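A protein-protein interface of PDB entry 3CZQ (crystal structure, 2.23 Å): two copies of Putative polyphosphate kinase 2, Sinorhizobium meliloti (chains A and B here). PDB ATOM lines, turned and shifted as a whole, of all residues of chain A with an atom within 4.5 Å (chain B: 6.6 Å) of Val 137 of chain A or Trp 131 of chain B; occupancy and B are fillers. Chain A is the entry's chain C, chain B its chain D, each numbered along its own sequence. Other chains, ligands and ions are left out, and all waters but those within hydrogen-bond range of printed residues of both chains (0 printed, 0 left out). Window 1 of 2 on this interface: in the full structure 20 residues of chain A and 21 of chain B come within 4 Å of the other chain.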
ATOM      1  N   ARG A  86       2.537  25.083  12.887  1.00  0.00           N
ATOM      2  CA  ARG A  86       3.598  25.709  12.126  1.00  0.00           C
ATOM      3  C   ARG A  86       3.295  25.614  10.638  1.00  0.00           C
ATOM      4  O   ARG A  86       2.832  24.577  10.147  1.00  0.00           O
ATOM      5  CB  ARG A  86       4.948  25.079  12.457  1.00  0.00           C
ATOM      6  CG  ARG A  86       5.353  25.293  13.917  1.00  0.00           C
ATOM      7  CD  ARG A  86       6.404  24.303  14.419  1.00  0.00           C
ATOM      8  NE  ARG A  86       5.944  22.930  14.299  1.00  0.00           N
ATOM      9  CZ  ARG A  86       6.691  21.846  14.523  1.00  0.00           C
ATOM     10  NH1 ARG A  86       7.967  21.960  14.885  1.00  0.00           N
ATOM     11  NH2 ARG A  86       6.153  20.642  14.361  1.00  0.00           N
ATOM     12  N   TRP A 131      25.819  20.196   3.959  1.00  0.00           N
ATOM     13  CA  TRP A 131      24.552  19.696   3.472  1.00  0.00           C
ATOM     14  C   TRP A 131      23.726  20.871   2.940  1.00  0.00           C
ATOM     15  O   TRP A 131      23.412  21.818   3.694  1.00  0.00           O
ATOM     16  CB  TRP A 131      23.813  19.016   4.612  1.00  0.00           C
ATOM     17  CG  TRP A 131      22.513  18.369   4.228  1.00  0.00           C
ATOM     18  CD1 TRP A 131      22.240  17.660   3.077  1.00  0.00           C
ATOM     19  CD2 TRP A 131      21.319  18.301   5.022  1.00  0.00           C
ATOM     20  NE1 TRP A 131      20.953  17.189   3.106  1.00  0.00           N
ATOM     21  CE2 TRP A 131      20.375  17.544   4.295  1.00  0.00           C
ATOM     22  CE3 TRP A 131      20.965  18.788   6.282  1.00  0.00           C
ATOM     23  CZ2 TRP A 131      19.095  17.295   4.778  1.00  0.00           C
ATOM     24  CZ3 TRP A 131      19.689  18.527   6.761  1.00  0.00           C
ATOM     25  CH2 TRP A 131      18.778  17.786   6.018  1.00  0.00           C
ATOM     26  N   PHE A 133      20.763  21.501   2.475  1.00  0.00           N
ATOM     27  CA  PHE A 133      19.563  21.873   3.212  1.00  0.00           C
ATOM     28  C   PHE A 133      19.829  22.496   4.568  1.00  0.00           C
ATOM     29  O   PHE A 133      18.896  22.998   5.198  1.00  0.00           O
ATOM     30  CB  PHE A 133      18.606  20.684   3.358  1.00  0.00           C
ATOM     31  CG  PHE A 133      18.026  20.207   2.043  1.00  0.00           C
ATOM     32  CD1 PHE A 133      16.899  20.825   1.494  1.00  0.00           C
ATOM     33  CD2 PHE A 133      18.614  19.148   1.353  1.00  0.00           C
ATOM     34  CE1 PHE A 133      16.358  20.388   0.262  1.00  0.00           C
ATOM     35  CE2 PHE A 133      18.079  18.699   0.111  1.00  0.00           C
ATOM     36  CZ  PHE A 133      16.960  19.323  -0.430  1.00  0.00           C
ATOM     37  N   GLN A 134      21.085  22.502   5.014  1.00  0.00           N
ATOM     38  CA  GLN A 134      21.395  22.892   6.399  1.00  0.00           C
ATOM     39  C   GLN A 134      20.881  24.293   6.736  1.00  0.00           C
ATOM     40  O   GLN A 134      20.192  24.495   7.748  1.00  0.00           O
ATOM     41  CB  GLN A 134      22.890  22.784   6.717  1.00  0.00           C
ATOM     42  CG  GLN A 134      23.144  23.017   8.194  1.00  0.00           C
ATOM     43  CD  GLN A 134      24.583  22.809   8.645  1.00  0.00           C
ATOM     44  OE1 GLN A 134      25.030  23.449   9.614  1.00  0.00           O
ATOM     45  NE2 GLN A 134      25.315  21.935   7.950  1.00  0.00           N
ATOM     46  N   ARG A 135      21.204  25.264   5.881  1.00  0.00           N
ATOM     47  CA  ARG A 135      20.907  26.652   6.198  1.00  0.00           C
ATOM     48  C   ARG A 135      19.394  26.966   6.086  1.00  0.00           C
ATOM     49  O   ARG A 135      18.895  27.929   6.682  1.00  0.00           O
ATOM     50  CB  ARG A 135      21.768  27.580   5.351  1.00  0.00           C
ATOM     51  CG  ARG A 135      21.388  27.617   3.890  1.00  0.00           C
ATOM     52  CD  ARG A 135      22.451  28.319   3.090  1.00  0.00           C
ATOM     53  NE  ARG A 135      21.962  28.712   1.768  1.00  0.00           N
ATOM     54  CZ  ARG A 135      21.942  29.959   1.308  1.00  0.00           C
ATOM     55  NH1 ARG A 135      21.480  30.202   0.085  1.00  0.00           N
ATOM     56  NH2 ARG A 135      22.399  30.961   2.053  1.00  0.00           N
ATOM     57  N   TYR A 136      18.669  26.131   5.359  1.00  0.00           N
ATOM     58  CA  TYR A 136      17.207  26.204   5.321  1.00  0.00           C
ATOM     59  C   TYR A 136      16.628  25.676   6.626  1.00  0.00           C
ATOM     60  O   TYR A 136      15.796  26.322   7.249  1.00  0.00           O
ATOM     61  CB  TYR A 136      16.665  25.478   4.082  1.00  0.00           C
ATOM     62  CG  TYR A 136      17.209  26.152   2.849  1.00  0.00           C
ATOM     63  CD1 TYR A 136      16.648  27.353   2.380  1.00  0.00           C
ATOM     64  CD2 TYR A 136      18.345  25.651   2.199  1.00  0.00           C
ATOM     65  CE1 TYR A 136      17.174  28.006   1.286  1.00  0.00           C
ATOM     66  CE2 TYR A 136      18.875  26.309   1.098  1.00  0.00           C
ATOM     67  CZ  TYR A 136      18.284  27.481   0.651  1.00  0.00           C
ATOM     68  OH  TYR A 136      18.798  28.125  -0.450  1.00  0.00           O
ATOM     69  N   VAL A 137      17.119  24.522   7.064  1.00  0.00           N
ATOM     70  CA  VAL A 137      16.760  23.987   8.387  1.00  0.00           C
ATOM     71  C   VAL A 137      16.888  25.030   9.514  1.00  0.00           C
ATOM     72  O   VAL A 137      15.984  25.123  10.337  1.00  0.00           O
ATOM     73  CB  VAL A 137      17.542  22.696   8.727  1.00  0.00           C
ATOM     74  CG1 VAL A 137      17.147  22.165  10.123  1.00  0.00           C
ATOM     75  CG2 VAL A 137      17.310  21.648   7.625  1.00  0.00           C
ATOM     76  N   ALA A 138      17.964  25.819   9.530  1.00  0.00           N
ATOM     77  CA  ALA A 138      18.172  26.842  10.583  1.00  0.00           C
ATOM     78  C   ALA A 138      17.039  27.859  10.749  1.00  0.00           C
ATOM     79  O   ALA A 138      16.900  28.473  11.802  1.00  0.00           O
ATOM     80  CB  ALA A 138      19.488  27.580  10.362  1.00  0.00           C
ATOM     81  N   THR A 139      16.241  28.020   9.691  1.00  0.00           N
ATOM     82  CA  THR A 139      15.175  29.019   9.601  1.00  0.00           C
ATOM     83  C   THR A 139      13.799  28.375   9.814  1.00  0.00           C
ATOM     84  O   THR A 139      12.774  29.062   9.760  1.00  0.00           O
ATOM     85  CB  THR A 139      15.152  29.703   8.193  1.00  0.00           C
ATOM     86  OG1 THR A 139      14.600  28.794   7.229  1.00  0.00           O
ATOM     87  CG2 THR A 139      16.549  30.131   7.740  1.00  0.00           C
ATOM     88  N   PHE A 140      13.780  27.061  10.020  1.00  0.00           N
ATOM     89  CA  PHE A 140      12.535  26.331  10.232  1.00  0.00           C
ATOM     90  C   PHE A 140      11.735  26.903  11.426  1.00  0.00           C
ATOM     91  O   PHE A 140      12.331  27.423  12.376  1.00  0.00           O
ATOM     92  CB  PHE A 140      12.831  24.842  10.458  1.00  0.00           C
ATOM     93  CG  PHE A 140      12.877  24.003   9.195  1.00  0.00           C
ATOM     94  CD1 PHE A 140      13.364  24.514   8.002  1.00  0.00           C
ATOM     95  CD2 PHE A 140      12.498  22.664   9.238  1.00  0.00           C
ATOM     96  CE1 PHE A 140      13.435  23.724   6.857  1.00  0.00           C
ATOM     97  CE2 PHE A 140      12.572  21.861   8.104  1.00  0.00           C
ATOM     98  CZ  PHE A 140      13.033  22.404   6.907  1.00  0.00           C
ATOM     99  N   PHE A 181      13.273  15.434   1.941  1.00  0.00           N
ATOM    100  CA  PHE A 181      13.311  16.612   2.801  1.00  0.00           C
ATOM    101  C   PHE A 181      11.913  17.059   3.210  1.00  0.00           C
ATOM    102  O   PHE A 181      11.649  17.280   4.399  1.00  0.00           O
ATOM    103  CB  PHE A 181      14.032  17.741   2.070  1.00  0.00           C
ATOM    104  CG  PHE A 181      14.281  18.966   2.914  1.00  0.00           C
ATOM    105  CD1 PHE A 181      15.227  18.952   3.928  1.00  0.00           C
ATOM    106  CD2 PHE A 181      13.591  20.152   2.658  1.00  0.00           C
ATOM    107  CE1 PHE A 181      15.461  20.090   4.683  1.00  0.00           C
ATOM    108  CE2 PHE A 181      13.818  21.288   3.412  1.00  0.00           C
ATOM    109  CZ  PHE A 181      14.754  21.263   4.413  1.00  0.00           C
ATOM    110  N   MET A 184       9.929  14.760   5.550  1.00  0.00           N
ATOM    111  CA  MET A 184      10.334  15.042   6.938  1.00  0.00           C
ATOM    112  C   MET A 184       9.587  16.207   7.561  1.00  0.00           C
ATOM    113  O   MET A 184       9.219  16.142   8.738  1.00  0.00           O
ATOM    114  CB  MET A 184      11.855  15.234   7.053  1.00  0.00           C
ATOM    115  CG  MET A 184      12.636  13.927   6.775  1.00  0.00           C
ATOM    116  SD  MET A 184      14.378  13.696   7.623  1.00  0.00           S
ATOM    117  CE  MET A 184      13.771  12.999   9.345  1.00  0.00           C
ATOM    118  N   GLU A 188       6.825  15.883  10.466  1.00  0.00           N
ATOM    119  CA  GLU A 188       6.945  16.752  11.627  1.00  0.00           C
ATOM    120  C   GLU A 188       5.612  17.463  11.938  1.00  0.00           C
ATOM    121  O   GLU A 188       5.341  17.837  13.087  1.00  0.00           O
ATOM    122  CB  GLU A 188       8.099  17.756  11.406  1.00  0.00           C
ATOM    123  CG  GLU A 188       8.272  18.838  12.472  1.00  0.00           C
ATOM    124  CD  GLU A 188       8.493  18.258  13.852  1.00  0.00           C
ATOM    125  OE1 GLU A 188       9.256  17.284  13.972  1.00  0.00           O
ATOM    126  OE2 GLU A 188       7.924  18.785  14.825  1.00  0.00           O
ATOM    127  N   GLU B 127      13.703  25.656  20.899  1.00  0.00           N
ATOM    128  CA  GLU B 127      14.131  24.352  20.365  1.00  0.00           C
ATOM    129  C   GLU B 127      13.117  23.211  20.582  1.00  0.00           C
ATOM    130  O   GLU B 127      13.094  22.222  19.832  1.00  0.00           O
ATOM    131  CB  GLU B 127      15.470  23.939  20.959  1.00  0.00           C
ATOM    132  CG  GLU B 127      16.646  24.825  20.537  1.00  0.00           C
ATOM    133  CD  GLU B 127      17.919  24.529  21.347  1.00  0.00           C
ATOM    134  OE1 GLU B 127      17.774  24.108  22.521  1.00  0.00           O
ATOM    135  OE2 GLU B 127      19.044  24.708  20.815  1.00  0.00           O
ATOM    136  N   ARG B 128      12.290  23.355  21.616  1.00  0.00           N
ATOM    137  CA  ARG B 128      11.272  22.368  21.960  1.00  0.00           C
ATOM    138  C   ARG B 128      10.046  22.417  21.049  1.00  0.00           C
ATOM    139  O   ARG B 128       9.372  21.406  20.857  1.00  0.00           O
ATOM    140  CB  ARG B 128      10.858  22.512  23.424  1.00  0.00           C
ATOM    141  CG  ARG B 128      11.550  21.518  24.350  1.00  0.00           C
ATOM    142  CD  ARG B 128      10.810  21.366  25.693  1.00  0.00           C
ATOM    143  NE  ARG B 128      10.356  22.660  26.217  1.00  0.00           N
ATOM    144  CZ  ARG B 128      11.005  23.383  27.133  1.00  0.00           C
ATOM    145  NH1 ARG B 128      12.145  22.939  27.659  1.00  0.00           N
ATOM    146  NH2 ARG B 128      10.503  24.557  27.527  1.00  0.00           N
ATOM    147  N   GLY B 129       9.759  23.595  20.499  1.00  0.00           N
ATOM    148  CA  GLY B 129       8.635  23.769  19.580  1.00  0.00           C
ATOM    149  C   GLY B 129       9.012  23.533  18.126  1.00  0.00           C
ATOM    150  O   GLY B 129       8.172  23.688  17.237  1.00  0.00           O
ATOM    151  N   GLN B 130      10.267  23.127  17.911  1.00  0.00           N
ATOM    152  CA  GLN B 130      10.871  22.941  16.587  1.00  0.00           C
ATOM    153  C   GLN B 130      10.925  21.486  16.155  1.00  0.00           C
ATOM    154  O   GLN B 130      10.808  20.570  16.976  1.00  0.00           O
ATOM    155  CB  GLN B 130      12.323  23.432  16.598  1.00  0.00           C
ATOM    156  CG  GLN B 130      12.521  24.915  16.755  1.00  0.00           C
ATOM    157  CD  GLN B 130      13.979  25.310  16.880  1.00  0.00           C
ATOM    158  OE1 GLN B 130      14.869  24.463  17.026  1.00  0.00           O
ATOM    159  NE2 GLN B 130      14.232  26.617  16.848  1.00  0.00           N
ATOM    160  N   TRP B 131      11.138  21.280  14.857  1.00  0.00           N
ATOM    161  CA  TRP B 131      11.597  20.004  14.363  1.00  0.00           C
ATOM    162  C   TRP B 131      12.616  19.464  15.356  1.00  0.00           C
ATOM    163  O   TRP B 131      13.523  20.189  15.742  1.00  0.00           O
ATOM    164  CB  TRP B 131      12.277  20.169  13.012  1.00  0.00           C
ATOM    165  CG  TRP B 131      12.525  18.871  12.288  1.00  0.00           C
ATOM    166  CD1 TRP B 131      11.773  17.722  12.370  1.00  0.00           C
ATOM    167  CD2 TRP B 131      13.560  18.601  11.331  1.00  0.00           C
ATOM    168  NE1 TRP B 131      12.281  16.766  11.536  1.00  0.00           N
ATOM    169  CE2 TRP B 131      13.366  17.270  10.872  1.00  0.00           C
ATOM    170  CE3 TRP B 131      14.620  19.349  10.809  1.00  0.00           C
ATOM    171  CZ2 TRP B 131      14.212  16.661   9.936  1.00  0.00           C
ATOM    172  CZ3 TRP B 131      15.455  18.753   9.865  1.00  0.00           C
ATOM    173  CH2 TRP B 131      15.243  17.416   9.436  1.00  0.00           C
ATOM    174  N   TYR B 132      12.470  18.204  15.758  1.00  0.00           N
ATOM    175  CA  TYR B 132      13.388  17.602  16.721  1.00  0.00           C
ATOM    176  C   TYR B 132      14.836  17.649  16.237  1.00  0.00           C
ATOM    177  O   TYR B 132      15.761  17.840  17.032  1.00  0.00           O
ATOM    178  CB  TYR B 132      12.990  16.148  17.035  1.00  0.00           C
ATOM    179  CG  TYR B 132      13.910  15.501  18.057  1.00  0.00           C
ATOM    180  CD1 TYR B 132      13.784  15.794  19.414  1.00  0.00           C
ATOM    181  CD2 TYR B 132      14.928  14.629  17.669  1.00  0.00           C
ATOM    182  CE1 TYR B 132      14.628  15.232  20.354  1.00  0.00           C
ATOM    183  CE2 TYR B 132      15.774  14.048  18.613  1.00  0.00           C
ATOM    184  CZ  TYR B 132      15.617  14.364  19.955  1.00  0.00           C
ATOM    185  OH  TYR B 132      16.446  13.815  20.917  1.00  0.00           O
ATOM    186  N   PHE B 133      15.017  17.481  14.928  1.00  0.00           N
ATOM    187  CA  PHE B 133      16.346  17.355  14.345  1.00  0.00           C
ATOM    188  C   PHE B 133      17.015  18.686  14.022  1.00  0.00           C
ATOM    189  O   PHE B 133      18.186  18.705  13.635  1.00  0.00           O
ATOM    190  CB  PHE B 133      16.291  16.484  13.094  1.00  0.00           C
ATOM    191  CG  PHE B 133      15.894  15.057  13.364  1.00  0.00           C
ATOM    192  CD1 PHE B 133      16.827  14.142  13.876  1.00  0.00           C
ATOM    193  CD2 PHE B 133      14.588  14.617  13.113  1.00  0.00           C
ATOM    194  CE1 PHE B 133      16.464  12.791  14.136  1.00  0.00           C
ATOM    195  CE2 PHE B 133      14.205  13.270  13.383  1.00  0.00           C
ATOM    196  CZ  PHE B 133      15.150  12.358  13.895  1.00  0.00           C
ATOM    197  N   GLN B 134      16.276  19.791  14.177  1.00  0.00           N
ATOM    198  CA  GLN B 134      16.775  21.123  13.820  1.00  0.00           C
ATOM    199  C   GLN B 134      18.093  21.504  14.529  1.00  0.00           C
ATOM    200  O   GLN B 134      19.069  21.835  13.859  1.00  0.00           O
ATOM    201  CB  GLN B 134      15.703  22.195  14.052  1.00  0.00           C
ATOM    202  CG  GLN B 134      16.084  23.585  13.466  1.00  0.00           C
ATOM    203  CD  GLN B 134      14.937  24.559  13.415  1.00  0.00           C
ATOM    204  OE1 GLN B 134      15.144  25.765  13.445  1.00  0.00           O
ATOM    205  NE2 GLN B 134      13.715  24.043  13.322  1.00  0.00           N
ATOM    206  N   ARG B 135      18.131  21.430  15.865  1.00  0.00           N
ATOM    207  CA  ARG B 135      19.323  21.838  16.625  1.00  0.00           C
ATOM    208  C   ARG B 135      20.562  20.949  16.389  1.00  0.00           C
ATOM    209  O   ARG B 135      21.701  21.410  16.523  1.00  0.00           O
ATOM    210  CB  ARG B 135      18.996  21.935  18.122  1.00  0.00           C
ATOM    211  CG  ARG B 135      18.881  20.598  18.809  1.00  0.00           C
ATOM    212  CD  ARG B 135      17.877  20.645  19.922  1.00  0.00           C
ATOM    213  NE  ARG B 135      18.485  21.020  21.188  1.00  0.00           N
ATOM    214  CZ  ARG B 135      18.958  20.169  22.089  1.00  0.00           C
ATOM    215  NH1 ARG B 135      18.910  18.862  21.883  1.00  0.00           N
ATOM    216  NH2 ARG B 135      19.490  20.627  23.205  1.00  0.00           N
ATOM    217  N   VAL B 137      21.053  19.497  13.337  1.00  0.00           N
ATOM    218  CA  VAL B 137      21.472  19.858  11.973  1.00  0.00           C
ATOM    219  C   VAL B 137      22.365  21.108  12.012  1.00  0.00           C
ATOM    220  O   VAL B 137      23.319  21.215  11.248  1.00  0.00           O
ATOM    221  CB  VAL B 137      20.261  20.008  11.002  1.00  0.00           C
ATOM    222  CG1 VAL B 137      20.697  20.635   9.674  1.00  0.00           C
ATOM    223  CG2 VAL B 137      19.588  18.657  10.772  1.00  0.00           C
ATOM    224  N   ALA B 138      22.070  22.025  12.930  1.00  0.00           N
ATOM    225  CA  ALA B 138      22.900  23.226  13.165  1.00  0.00           C
ATOM    226  C   ALA B 138      24.377  22.911  13.387  1.00  0.00           C
ATOM    227  O   ALA B 138      25.226  23.764  13.236  1.00  0.00           O
ATOM    228  CB  ALA B 138      22.358  24.019  14.369  1.00  0.00           C
ATOM    229  N   GLU B 177      11.354   8.290  12.332  1.00  0.00           N
ATOM    230  CA  GLU B 177      12.009   9.381  11.583  1.00  0.00           C
ATOM    231  C   GLU B 177      13.534   9.349  11.489  1.00  0.00           C
ATOM    232  O   GLU B 177      14.091   9.874  10.526  1.00  0.00           O
ATOM    233  CB  GLU B 177      11.535  10.767  12.057  1.00  0.00           C
ATOM    234  CG  GLU B 177      10.069  11.076  11.726  1.00  0.00           C
ATOM    235  CD  GLU B 177       9.768  11.049  10.222  1.00  0.00           C
ATOM    236  OE1 GLU B 177      10.426  11.775   9.444  1.00  0.00           O
ATOM    237  OE2 GLU B 177       8.854  10.301   9.814  1.00  0.00           O
ATOM    238  N   PHE B 181      16.210  10.428   8.456  1.00  0.00           N
ATOM    239  CA  PHE B 181      17.244  11.435   8.752  1.00  0.00           C
ATOM    240  C   PHE B 181      18.618  10.933   8.323  1.00  0.00           C
ATOM    241  O   PHE B 181      19.347  11.603   7.600  1.00  0.00           O
ATOM    242  CB  PHE B 181      17.235  11.728  10.254  1.00  0.00           C
ATOM    243  CG  PHE B 181      18.121  12.886  10.680  1.00  0.00           C
ATOM    244  CD1 PHE B 181      17.907  14.174  10.190  1.00  0.00           C
ATOM    245  CD2 PHE B 181      19.127  12.690  11.630  1.00  0.00           C
ATOM    246  CE1 PHE B 181      18.709  15.237  10.611  1.00  0.00           C
ATOM    247  CE2 PHE B 181      19.934  13.755  12.052  1.00  0.00           C
ATOM    248  CZ  PHE B 181      19.720  15.021  11.549  1.00  0.00           C
ATOM    249  N   MET B 184      19.186  10.730   4.504  1.00  0.00           N
ATOM    250  CA  MET B 184      19.622  12.012   3.936  1.00  0.00           C
ATOM    251  C   MET B 184      21.077  12.365   4.265  1.00  0.00           C
ATOM    252  O   MET B 184      21.766  12.977   3.441  1.00  0.00           O
ATOM    253  CB  MET B 184      18.701  13.186   4.346  1.00  0.00           C
ATOM    254  CG  MET B 184      17.222  13.022   4.001  1.00  0.00           C
ATOM    255  SD  MET B 184      16.186  14.692   4.097  1.00  0.00           S
ATOM    256  CE  MET B 184      16.889  15.532   2.478  1.00  0.00           C
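OE1 of Gln 134 of chain B sits close to O of Phe 140 of chain A (3.4 Å).
The guanidinium group (NH1) of Arg 86 of chain A lies within hydrogen-bond range of the backbone carbonyl oxygen (O) of Gly 129 of chain B (2.9 Å).
NH1 of Arg 86 of chain A lies close to N of Trp 131 of chain B (3.2 Å).
The backbone carbonyl oxygen of Val 137 of chain B lies close to the side-chain amide oxygen of Gln 134 of chain A.
The side-chain sulfur of Met 184 of chain B sits close to the backbone NH of Phe 181 of chain A (3.7 Å).
OE1 of Gln 134 of chain B lies close to O of Val 137 of chain A.
NH2 of Arg 86 of chain A is in salt-bridge range of OE2 of Glu 188 of chain A, 2.6 Å away.
Arg 86 of chain A touches Gln 130 of chain B (NH1 to C, 3.3 Å).
Trp 131 of chain A touches Val 137 of chain B.
Gln 134 of chain A touches Ala 138 of chain B.
Trp 131 of chain B touches Val 137 of chain A (CZ3 to CG1, 3.8 Å).
Val 137 of chain B touches Val 137 of chain A.
Met 184 of chain A touches Trp 131 of chain B.
Met 184 of chain A touches Glu 177 of chain B (CE to O, 3.4 Å).
Phe 181 of chain B touches Met 184 of chain A.
Glu 188 of chain A touches Trp 131 of chain B.
OE1 of Glu 188 of chain A touches N of Tyr 132 of chain B, 3.8 Å away.
Printed residues of chain B within 4 Å of Gln 134 of chain A: Val 137 (3.3 Å) and Ala 138 (3.6 Å).
Arg 135 of chain A touches none of the printed residues of chain B.
Val 137 of chain A touches three residues of chain B.
Arg 128 of chain B touches none of the printed residues of chain A.
Of the printed residues of chain A, Gly 129 of chain B touches Arg 86.
Of the printed residues of chain A, Trp 131 of chain B touches Arg 86 (3.2 Å), Val 137 (3.8 Å), Met 184 (3.7 Å) and Glu 188 (3.0 Å).
Of the printed residues of chain A, Met 184 of chain B touches Trp 131 and Phe 181.
The nearest residue of chain B that does not touch Val 137 of chain A is Phe 133 of chain B (5.0 Å).
The nearest printed residue of chain A that does not touch Phe 181 of chain B is Trp 131 of chain A (5.2 Å).
Of the 13 printed residues of chain A, 9 touch a printed residue of chain B.
Hydrophobic or aromatic side chains of chain A that line the printed part of chain B: Trp 131, Val 137, Phe 140, Phe 181 and Met 184.
Along chain B the printed residues that touch a printed residue of chain A span positions 129 to 184.
Among the printed residues, 18 pairs touch across the chains.
Among the printed residues, no Asp or Glu carboxylate lies within 4 Å of a Lys or Arg side-chain nitrogen of the other chain.
Trp 131 of chain A touches Val 137 of chain B, and with the chains exchanged Val 137 of chain A touches Trp 131 of chain B.
Trp 131 of chain A touches Met 184 of chain B, and with the chains exchanged Met 184 of chain A touches Trp 131 of chain B.
Gln 134 of chain A touches Val 137 of chain B, and with the chains exchanged Val 137 of chain A touches Gln 134 of chain B.
Val 137 of chain B touches its own counterpart, Val 137 of chain A.
Positions printed for both chains: 131, 133, 134, 135, 137, 138, 181 and 184.
Of the 18 pairs that touch across the chains among the printed residues, 11 have their exchanged pair printed and touching as well.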
